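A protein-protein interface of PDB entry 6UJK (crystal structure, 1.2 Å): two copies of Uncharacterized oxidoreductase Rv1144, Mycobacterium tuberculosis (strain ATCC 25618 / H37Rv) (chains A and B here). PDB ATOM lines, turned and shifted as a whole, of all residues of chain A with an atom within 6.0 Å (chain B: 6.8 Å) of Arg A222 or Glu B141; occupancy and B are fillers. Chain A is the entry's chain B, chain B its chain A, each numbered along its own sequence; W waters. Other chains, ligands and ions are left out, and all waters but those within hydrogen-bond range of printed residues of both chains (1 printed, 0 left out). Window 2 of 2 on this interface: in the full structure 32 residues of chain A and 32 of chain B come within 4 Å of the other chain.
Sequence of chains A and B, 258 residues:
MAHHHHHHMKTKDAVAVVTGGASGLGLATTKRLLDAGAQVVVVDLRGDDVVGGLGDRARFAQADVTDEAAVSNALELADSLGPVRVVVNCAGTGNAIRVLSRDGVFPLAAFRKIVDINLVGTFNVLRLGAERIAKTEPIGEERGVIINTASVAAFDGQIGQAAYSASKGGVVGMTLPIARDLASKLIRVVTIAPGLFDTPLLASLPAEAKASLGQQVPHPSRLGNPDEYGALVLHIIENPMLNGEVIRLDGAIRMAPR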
ATOM      1  N   LEU A 196      -8.890   3.903   8.841  1.00  0.00           N
ATOM      2  CA  LEU A 196      -8.507   3.937   7.428  1.00  0.00           C
ATOM      3  C   LEU A 196      -8.942   5.248   6.785  1.00  0.00           C
ATOM      4  O   LEU A 196     -10.140   5.541   6.737  1.00  0.00           O
ATOM      5  CB  LEU A 196      -9.136   2.757   6.688  1.00  0.00           C
ATOM      6  CG  LEU A 196      -8.826   1.382   7.289  1.00  0.00           C
ATOM      7  CD1 LEU A 196      -9.707   0.316   6.644  1.00  0.00           C
ATOM      8  CD2 LEU A 196      -7.349   1.023   7.203  1.00  0.00           C
ATOM      9  N   GLY A 214     -12.686  -0.020   2.282  1.00  0.00           N
ATOM     10  CA  GLY A 214     -13.731   0.799   2.870  1.00  0.00           C
ATOM     11  C   GLY A 214     -14.969   0.013   3.246  1.00  0.00           C
ATOM     12  O   GLY A 214     -15.640   0.341   4.229  1.00  0.00           O
ATOM     13  N   GLN A 215     -15.282  -1.041   2.490  1.00  0.00           N
ATOM     14  CA  GLN A 215     -16.458  -1.845   2.786  1.00  0.00           C
ATOM     15  C   GLN A 215     -16.367  -2.534   4.134  1.00  0.00           C
ATOM     16  O   GLN A 215     -17.409  -2.862   4.713  1.00  0.00           O
ATOM     17  CB  GLN A 215     -16.647  -2.912   1.715  1.00  0.00           C
ATOM     18  N   VAL A 217     -15.274  -1.153   6.854  1.00  0.00           N
ATOM     19  CA  VAL A 217     -15.534  -0.219   7.952  1.00  0.00           C
ATOM     20  C   VAL A 217     -17.020  -0.304   8.300  1.00  0.00           C
ATOM     21  O   VAL A 217     -17.861  -0.162   7.395  1.00  0.00           O
ATOM     22  CB  VAL A 217     -15.154   1.205   7.535  1.00  0.00           C
ATOM     23  CG1 VAL A 217     -15.433   2.180   8.683  1.00  0.00           C
ATOM     24  CG2 VAL A 217     -13.715   1.285   7.039  1.00  0.00           C
ATOM     25  N   HIS A 219     -19.427   1.655   9.833  1.00  0.00           N
ATOM     26  CA  HIS A 219     -20.243   2.791   9.418  1.00  0.00           C
ATOM     27  C   HIS A 219     -19.520   4.062   9.830  1.00  0.00           C
ATOM     28  O   HIS A 219     -19.171   4.217  11.007  1.00  0.00           O
ATOM     29  CB  HIS A 219     -21.646   2.730  10.039  1.00  0.00           C
ATOM     30  CG  HIS A 219     -22.463   3.956   9.803  1.00  0.00           C
ATOM     31  ND1 HIS A 219     -22.739   4.456   8.544  1.00  0.00           N
ATOM     32  CD2 HIS A 219     -23.080   4.775  10.687  1.00  0.00           C
ATOM     33  CE1 HIS A 219     -23.446   5.566   8.674  1.00  0.00           C
ATOM     34  NE2 HIS A 219     -23.693   5.763   9.960  1.00  0.00           N
ATOM     35  N   PRO A 220     -19.232   4.996   8.906  1.00  0.00           N
ATOM     36  CA  PRO A 220     -19.559   4.919   7.473  1.00  0.00           C
ATOM     37  C   PRO A 220     -18.656   3.931   6.746  1.00  0.00           C
ATOM     38  O   PRO A 220     -17.456   3.845   7.016  1.00  0.00           O
ATOM     39  CB  PRO A 220     -19.303   6.345   6.990  1.00  0.00           C
ATOM     40  CG  PRO A 220     -18.198   6.816   7.862  1.00  0.00           C
ATOM     41  CD  PRO A 220     -18.388   6.167   9.219  1.00  0.00           C
ATOM     42  N   SER A 221     -19.246   3.166   5.833  1.00  0.00           N
ATOM     43  CA  SER A 221     -18.525   2.085   5.167  1.00  0.00           C
ATOM     44  C   SER A 221     -17.736   2.632   3.981  1.00  0.00           C
ATOM     45  O   SER A 221     -18.033   2.375   2.817  1.00  0.00           O
ATOM     46  CB  SER A 221     -19.469   0.981   4.725  1.00  0.00           C
ATOM     47  OG  SER A 221     -20.183   0.443   5.818  1.00  0.00           O
ATOM     48  N   ARG A 222     -16.705   3.401   4.306  1.00  0.00           N
ATOM     49  CA  ARG A 222     -15.832   4.023   3.323  1.00  0.00           C
ATOM     50  C   ARG A 222     -14.548   4.413   4.038  1.00  0.00           C
ATOM     51  O   ARG A 222     -14.483   4.429   5.267  1.00  0.00           O
ATOM     52  CB  ARG A 222     -16.483   5.275   2.734  1.00  0.00           C
ATOM     53  CG  ARG A 222     -16.878   6.268   3.837  1.00  0.00           C
ATOM     54  CD  ARG A 222     -17.073   7.630   3.293  1.00  0.00           C
ATOM     55  NE  ARG A 222     -17.662   8.539   4.259  1.00  0.00           N
ATOM     56  CZ  ARG A 222     -17.001   9.346   5.092  1.00  0.00           C
ATOM     57  NH1 ARG A 222     -15.669   9.369   5.141  1.00  0.00           N
ATOM     58  NH2 ARG A 222     -17.697  10.145   5.889  1.00  0.00           N
ATOM     59  N   LEU A 223     -13.526   4.769   3.255  1.00  0.00           N
ATOM     60  CA  LEU A 223     -12.346   5.405   3.827  1.00  0.00           C
ATOM     61  C   LEU A 223     -12.705   6.763   4.417  1.00  0.00           C
ATOM     62  O   LEU A 223     -13.563   7.490   3.910  1.00  0.00           O
ATOM     63  CB  LEU A 223     -11.276   5.591   2.749  1.00  0.00           C
ATOM     64  CG  LEU A 223     -10.766   4.311   2.090  1.00  0.00           C
ATOM     65  CD1 LEU A 223      -9.792   4.686   0.989  1.00  0.00           C
ATOM     66  CD2 LEU A 223     -10.119   3.375   3.100  1.00  0.00           C
ATOM     67  N   GLY A 224     -12.013   7.114   5.489  1.00  0.00           N
ATOM     68  CA  GLY A 224     -12.166   8.438   6.055  1.00  0.00           C
ATOM     69  C   GLY A 224     -11.715   9.524   5.098  1.00  0.00           C
ATOM     70  O   GLY A 224     -10.773   9.357   4.320  1.00  0.00           O
ATOM     71  N   ASN A 225     -12.394  10.649   5.160  1.00  0.00           N
ATOM     72  CA  ASN A 225     -11.959  11.856   4.474  1.00  0.00           C
ATOM     73  C   ASN A 225     -10.994  12.610   5.379  1.00  0.00           C
ATOM     74  O   ASN A 225     -11.324  12.863   6.539  1.00  0.00           O
ATOM     75  CB  ASN A 225     -13.188  12.728   4.202  1.00  0.00           C
ATOM     76  CG  ASN A 225     -12.889  13.969   3.359  1.00  0.00           C
ATOM     77  OD1 ASN A 225     -11.910  14.672   3.575  1.00  0.00           O
ATOM     78  ND2 ASN A 225     -13.747  14.234   2.384  1.00  0.00           N
ATOM     79  N   GLU A 228     -12.185  15.044   8.021  1.00  0.00           N
ATOM     80  CA  GLU A 228     -12.795  14.600   9.278  1.00  0.00           C
ATOM     81  C   GLU A 228     -11.756  14.511  10.388  1.00  0.00           C
ATOM     82  O   GLU A 228     -12.067  14.732  11.568  1.00  0.00           O
ATOM     83  CB  GLU A 228     -13.512  13.260   9.053  1.00  0.00           C
ATOM     84  CG  GLU A 228     -14.712  13.475   8.098  1.00  0.00           C
ATOM     85  CD  GLU A 228     -15.233  12.272   7.352  1.00  0.00           C
ATOM     86  OE1 GLU A 228     -16.425  12.324   7.001  1.00  0.00           O
ATOM     87  OE2 GLU A 228     -14.510  11.301   7.052  1.00  0.00           O
ATOM     88  N   PRO B 138     -32.290   8.488   4.945  1.00  0.00           N
ATOM     89  CA  PRO B 138     -30.917   8.950   5.153  1.00  0.00           C
ATOM     90  C   PRO B 138     -30.733  10.357   4.608  1.00  0.00           C
ATOM     91  O   PRO B 138     -31.363  10.752   3.623  1.00  0.00           O
ATOM     92  CB  PRO B 138     -30.081   7.931   4.369  1.00  0.00           C
ATOM     93  CG  PRO B 138     -30.938   6.715   4.288  1.00  0.00           C
ATOM     94  CD  PRO B 138     -32.343   7.223   4.188  1.00  0.00           C
ATOM     95  N   ILE B 139     -29.855  11.117   5.259  1.00  0.00           N
ATOM     96  CA  ILE B 139     -29.336  12.362   4.707  1.00  0.00           C
ATOM     97  C   ILE B 139     -27.913  12.034   4.320  1.00  0.00           C
ATOM     98  O   ILE B 139     -27.061  11.785   5.184  1.00  0.00           O
ATOM     99  CB  ILE B 139     -29.402  13.539   5.684  1.00  0.00           C
ATOM    100  CG1 ILE B 139     -30.846  13.813   6.084  1.00  0.00           C
ATOM    101  CG2 ILE B 139     -28.786  14.791   5.040  1.00  0.00           C
ATOM    102  CD1 ILE B 139     -30.979  14.910   7.086  1.00  0.00           C
ATOM    103  N   GLY B 140     -27.682  11.948   3.023  1.00  0.00           N
ATOM    104  CA  GLY B 140     -26.450  11.371   2.534  1.00  0.00           C
ATOM    105  C   GLY B 140     -26.271   9.970   3.077  1.00  0.00           C
ATOM    106  O   GLY B 140     -27.104   9.073   2.902  1.00  0.00           O
ATOM    107  N   GLU B 141     -25.172   9.774   3.766  1.00  0.00           N
ATOM    108  CA  GLU B 141     -24.786   8.456   4.225  1.00  0.00           C
ATOM    109  C   GLU B 141     -25.257   8.141   5.636  1.00  0.00           C
ATOM    110  O   GLU B 141     -24.854   7.105   6.148  1.00  0.00           O
ATOM    111  CB  GLU B 141     -23.256   8.295   4.160  1.00  0.00           C
ATOM    112  CG  GLU B 141     -22.555   9.183   5.160  1.00  0.00           C
ATOM    113  CD  GLU B 141     -21.041   9.218   5.018  1.00  0.00           C
ATOM    114  OE1 GLU B 141     -20.456   8.458   4.195  1.00  0.00           O
ATOM    115  OE2 GLU B 141     -20.439  10.026   5.759  1.00  0.00           O
ATOM    116  N   GLU B 142     -26.047   9.003   6.290  1.00  0.00           N
ATOM    117  CA  GLU B 142     -26.344   8.825   7.713  1.00  0.00           C
ATOM    118  C   GLU B 142     -27.827   8.952   7.994  1.00  0.00           C
ATOM    119  O   GLU B 142     -28.492   9.805   7.415  1.00  0.00           O
ATOM    120  CB  GLU B 142     -25.634   9.890   8.566  1.00  0.00           C
ATOM    121  CG  GLU B 142     -24.123   9.828   8.565  1.00  0.00           C
ATOM    122  CD  GLU B 142     -23.529  10.770   9.606  1.00  0.00           C
ATOM    123  OE1 GLU B 142     -23.613  10.468  10.823  1.00  0.00           O
ATOM    124  OE2 GLU B 142     -22.977  11.820   9.210  1.00  0.00           O
ATOM    125  N   ARG B 143     -28.341   8.115   8.906  1.00  0.00           N
ATOM    126  CA  ARG B 143     -29.656   8.370   9.488  1.00  0.00           C
ATOM    127  C   ARG B 143     -29.558   9.142  10.800  1.00  0.00           C
ATOM    128  O   ARG B 143     -30.365  10.045  11.040  1.00  0.00           O
ATOM    129  CB  ARG B 143     -30.456   7.078   9.667  1.00  0.00           C
ATOM    130  CG  ARG B 143     -31.039   6.554   8.378  1.00  0.00           C
ATOM    131  CD  ARG B 143     -31.983   5.376   8.646  1.00  0.00           C
ATOM    132  NE  ARG B 143     -32.575   4.895   7.404  1.00  0.00           N
ATOM    133  CZ  ARG B 143     -31.991   4.025   6.594  1.00  0.00           C
ATOM    134  NH1 ARG B 143     -30.804   3.506   6.904  1.00  0.00           N
ATOM    135  NH2 ARG B 143     -32.583   3.686   5.445  1.00  0.00           N
ATOM    136  N   LYS B 185     -27.926   0.088   9.348  1.00  0.00           N
ATOM    137  CA  LYS B 185     -29.005   1.063   9.340  1.00  0.00           C
ATOM    138  C   LYS B 185     -28.517   2.498   9.421  1.00  0.00           C
ATOM    139  O   LYS B 185     -29.345   3.430   9.469  1.00  0.00           O
ATOM    140  CB  LYS B 185     -30.025   0.699  10.417  1.00  0.00           C
ATOM    141  CG  LYS B 185     -30.762  -0.603   9.994  1.00  0.00           C
ATOM    142  CD  LYS B 185     -31.705  -1.262  10.984  1.00  0.00           C
ATOM    143  CE  LYS B 185     -32.389  -2.491  10.304  1.00  0.00           C
ATOM    144  NZ  LYS B 185     -33.119  -3.382  11.219  1.00  0.00           N
ATOM    145  N   LEU B 186     -27.202   2.705   9.422  1.00  0.00           N
ATOM    146  CA  LEU B 186     -26.624   4.041   9.285  1.00  0.00           C
ATOM    147  C   LEU B 186     -26.841   4.882  10.545  1.00  0.00           C
ATOM    148  O   LEU B 186     -27.105   6.083  10.484  1.00  0.00           O
ATOM    149  CB  LEU B 186     -27.102   4.761   8.024  1.00  0.00           C
ATOM    150  CG  LEU B 186     -27.121   3.933   6.737  1.00  0.00           C
ATOM    151  CD1 LEU B 186     -27.635   4.780   5.574  1.00  0.00           C
ATOM    152  CD2 LEU B 186     -25.732   3.353   6.412  1.00  0.00           C
ATOM    153  N   ILE B 187     -26.676   4.241  11.704  1.00  0.00           N
ATOM    154  CA  ILE B 187     -26.777   4.903  12.996  1.00  0.00           C
ATOM    155  C   ILE B 187     -25.465   4.695  13.736  1.00  0.00           C
ATOM    156  O   ILE B 187     -25.092   3.552  14.018  1.00  0.00           O
ATOM    157  CB  ILE B 187     -27.945   4.367  13.836  1.00  0.00           C
ATOM    158  CG1 ILE B 187     -29.261   4.462  13.055  1.00  0.00           C
ATOM    159  CG2 ILE B 187     -28.015   5.125  15.169  1.00  0.00           C
ATOM    160  CD1 ILE B 187     -30.425   3.718  13.724  1.00  0.00           C
ATOM    161  N   PRO B 240     -18.636  12.414  10.967  1.00  0.00           N
ATOM    162  CA  PRO B 240     -19.152  11.093  10.582  1.00  0.00           C
ATOM    163  C   PRO B 240     -18.236   9.947  10.942  1.00  0.00           C
ATOM    164  O   PRO B 240     -18.709   8.811  10.980  1.00  0.00           O
ATOM    165  CB  PRO B 240     -19.304  11.201   9.054  1.00  0.00           C
ATOM    166  CG  PRO B 240     -19.471  12.639   8.804  1.00  0.00           C
ATOM    167  CD  PRO B 240     -18.578  13.328   9.815  1.00  0.00           C
ATOM    168  N   MET B 241     -16.947  10.174  11.190  1.00  0.00           N
ATOM    169  CA  MET B 241     -16.051   9.050  11.433  1.00  0.00           C
ATOM    170  C   MET B 241     -15.993   8.617  12.891  1.00  0.00           C
ATOM    171  O   MET B 241     -15.371   7.585  13.172  1.00  0.00           O
ATOM    172  CB  MET B 241     -14.646   9.377  10.917  1.00  0.00           C
ATOM    173  CG  MET B 241     -14.526   9.226   9.420  1.00  0.00           C
ATOM    174  SD  MET B 241     -14.606   7.513   8.882  1.00  0.00           S
ATOM    175  CE  MET B 241     -13.083   6.891   9.558  1.00  0.00           C
HETATM  176  O   HOH W   1     -24.784   8.088  11.209  1.00  0.00           O
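Water W1 lies within hydrogen-bond range of OE1 of Glu B142, NE2 of His A219 and O of Leu B186.
Of the 11 printed residues of chain B, 5 touch a printed residue of chain A.
Hydrophobic or aromatic side chains of chain B that line the printed part of chain A: Leu B186, Pro B240 and Met B241.
OE2 of Glu B141 is in salt-bridge range of NH2 of Arg A222, 2.7 Å away.
The backbone carbonyl oxygen (O) of Leu B186 lies close to a ring nitrogen (NE2) of His A219 (3.5 Å).
N of Arg B143 is in hydrogen-bond range of O of Leu B186.
The backbone NH of Gly A224 lies within hydrogen-bond range of the backbone carbonyl oxygen of Leu A196.
The backbone NH (N) of Arg A222 lies within hydrogen-bond range of the backbone carbonyl oxygen (O) of Gly A214 (3.2 Å).
The guanidinium group (NH2) of Arg A222 lies within salt-bridge range of the side-chain carboxylate (OE1) of Glu A228, at 2.8 Å.
N of Asn A225 lies within hydrogen-bond range of OE2 of Glu A228 (2.9 Å).
No position is printed for both chains.
Glu B141 touches His A219 (O to CE1, 3.3 Å).
N of Ile B187 touches CD2 of His A219, 3.8 Å away.
OE1 of Glu B141 touches CB of Pro A220, 3.7 Å away.
Pro A220 touches Pro B240 (CD to O, 3.2 Å).
Pro A220 touches Met B241 (CG to SD, 3.8 Å).
CB of Pro B240 touches NH2 of Arg A222, at 3.7 Å.
Gly A224 touches Met B241.
OE1 of Glu A228 touches CG of Pro B240, at 3.6 Å.
OE2 of Glu A228 touches CG of Met B241, 3.1 Å away.
Printed residues of chain B within 4 Å of His A219: Glu B141, Leu B186 and Ile B187.
Printed residues of chain B within 4 Å of Pro A220: Glu B141, Pro B240 and Met B241.
Ser A221 touches none of the printed residues of chain B.
Arg A222 touches just these residues of chain B: Glu B141 and Pro B240.
Asn A225 touches none of the printed residues of chain B.
Of the printed residues of chain A, Glu B141 touches His A219, Pro A220 and Arg A222.
Printed residues of chain A within 4 Å of Ile B187: His A219 (3.8 Å).
Of the printed residues of chain A, Pro B240 touches Pro A220, Arg A222 and Glu A228.
Of the printed residues of chain A, Met B241 touches Pro A220, Gly A224 and Glu A228.
The nearest printed residue of chain B that does not touch Glu A228 is Glu B141 (4.8 Å).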
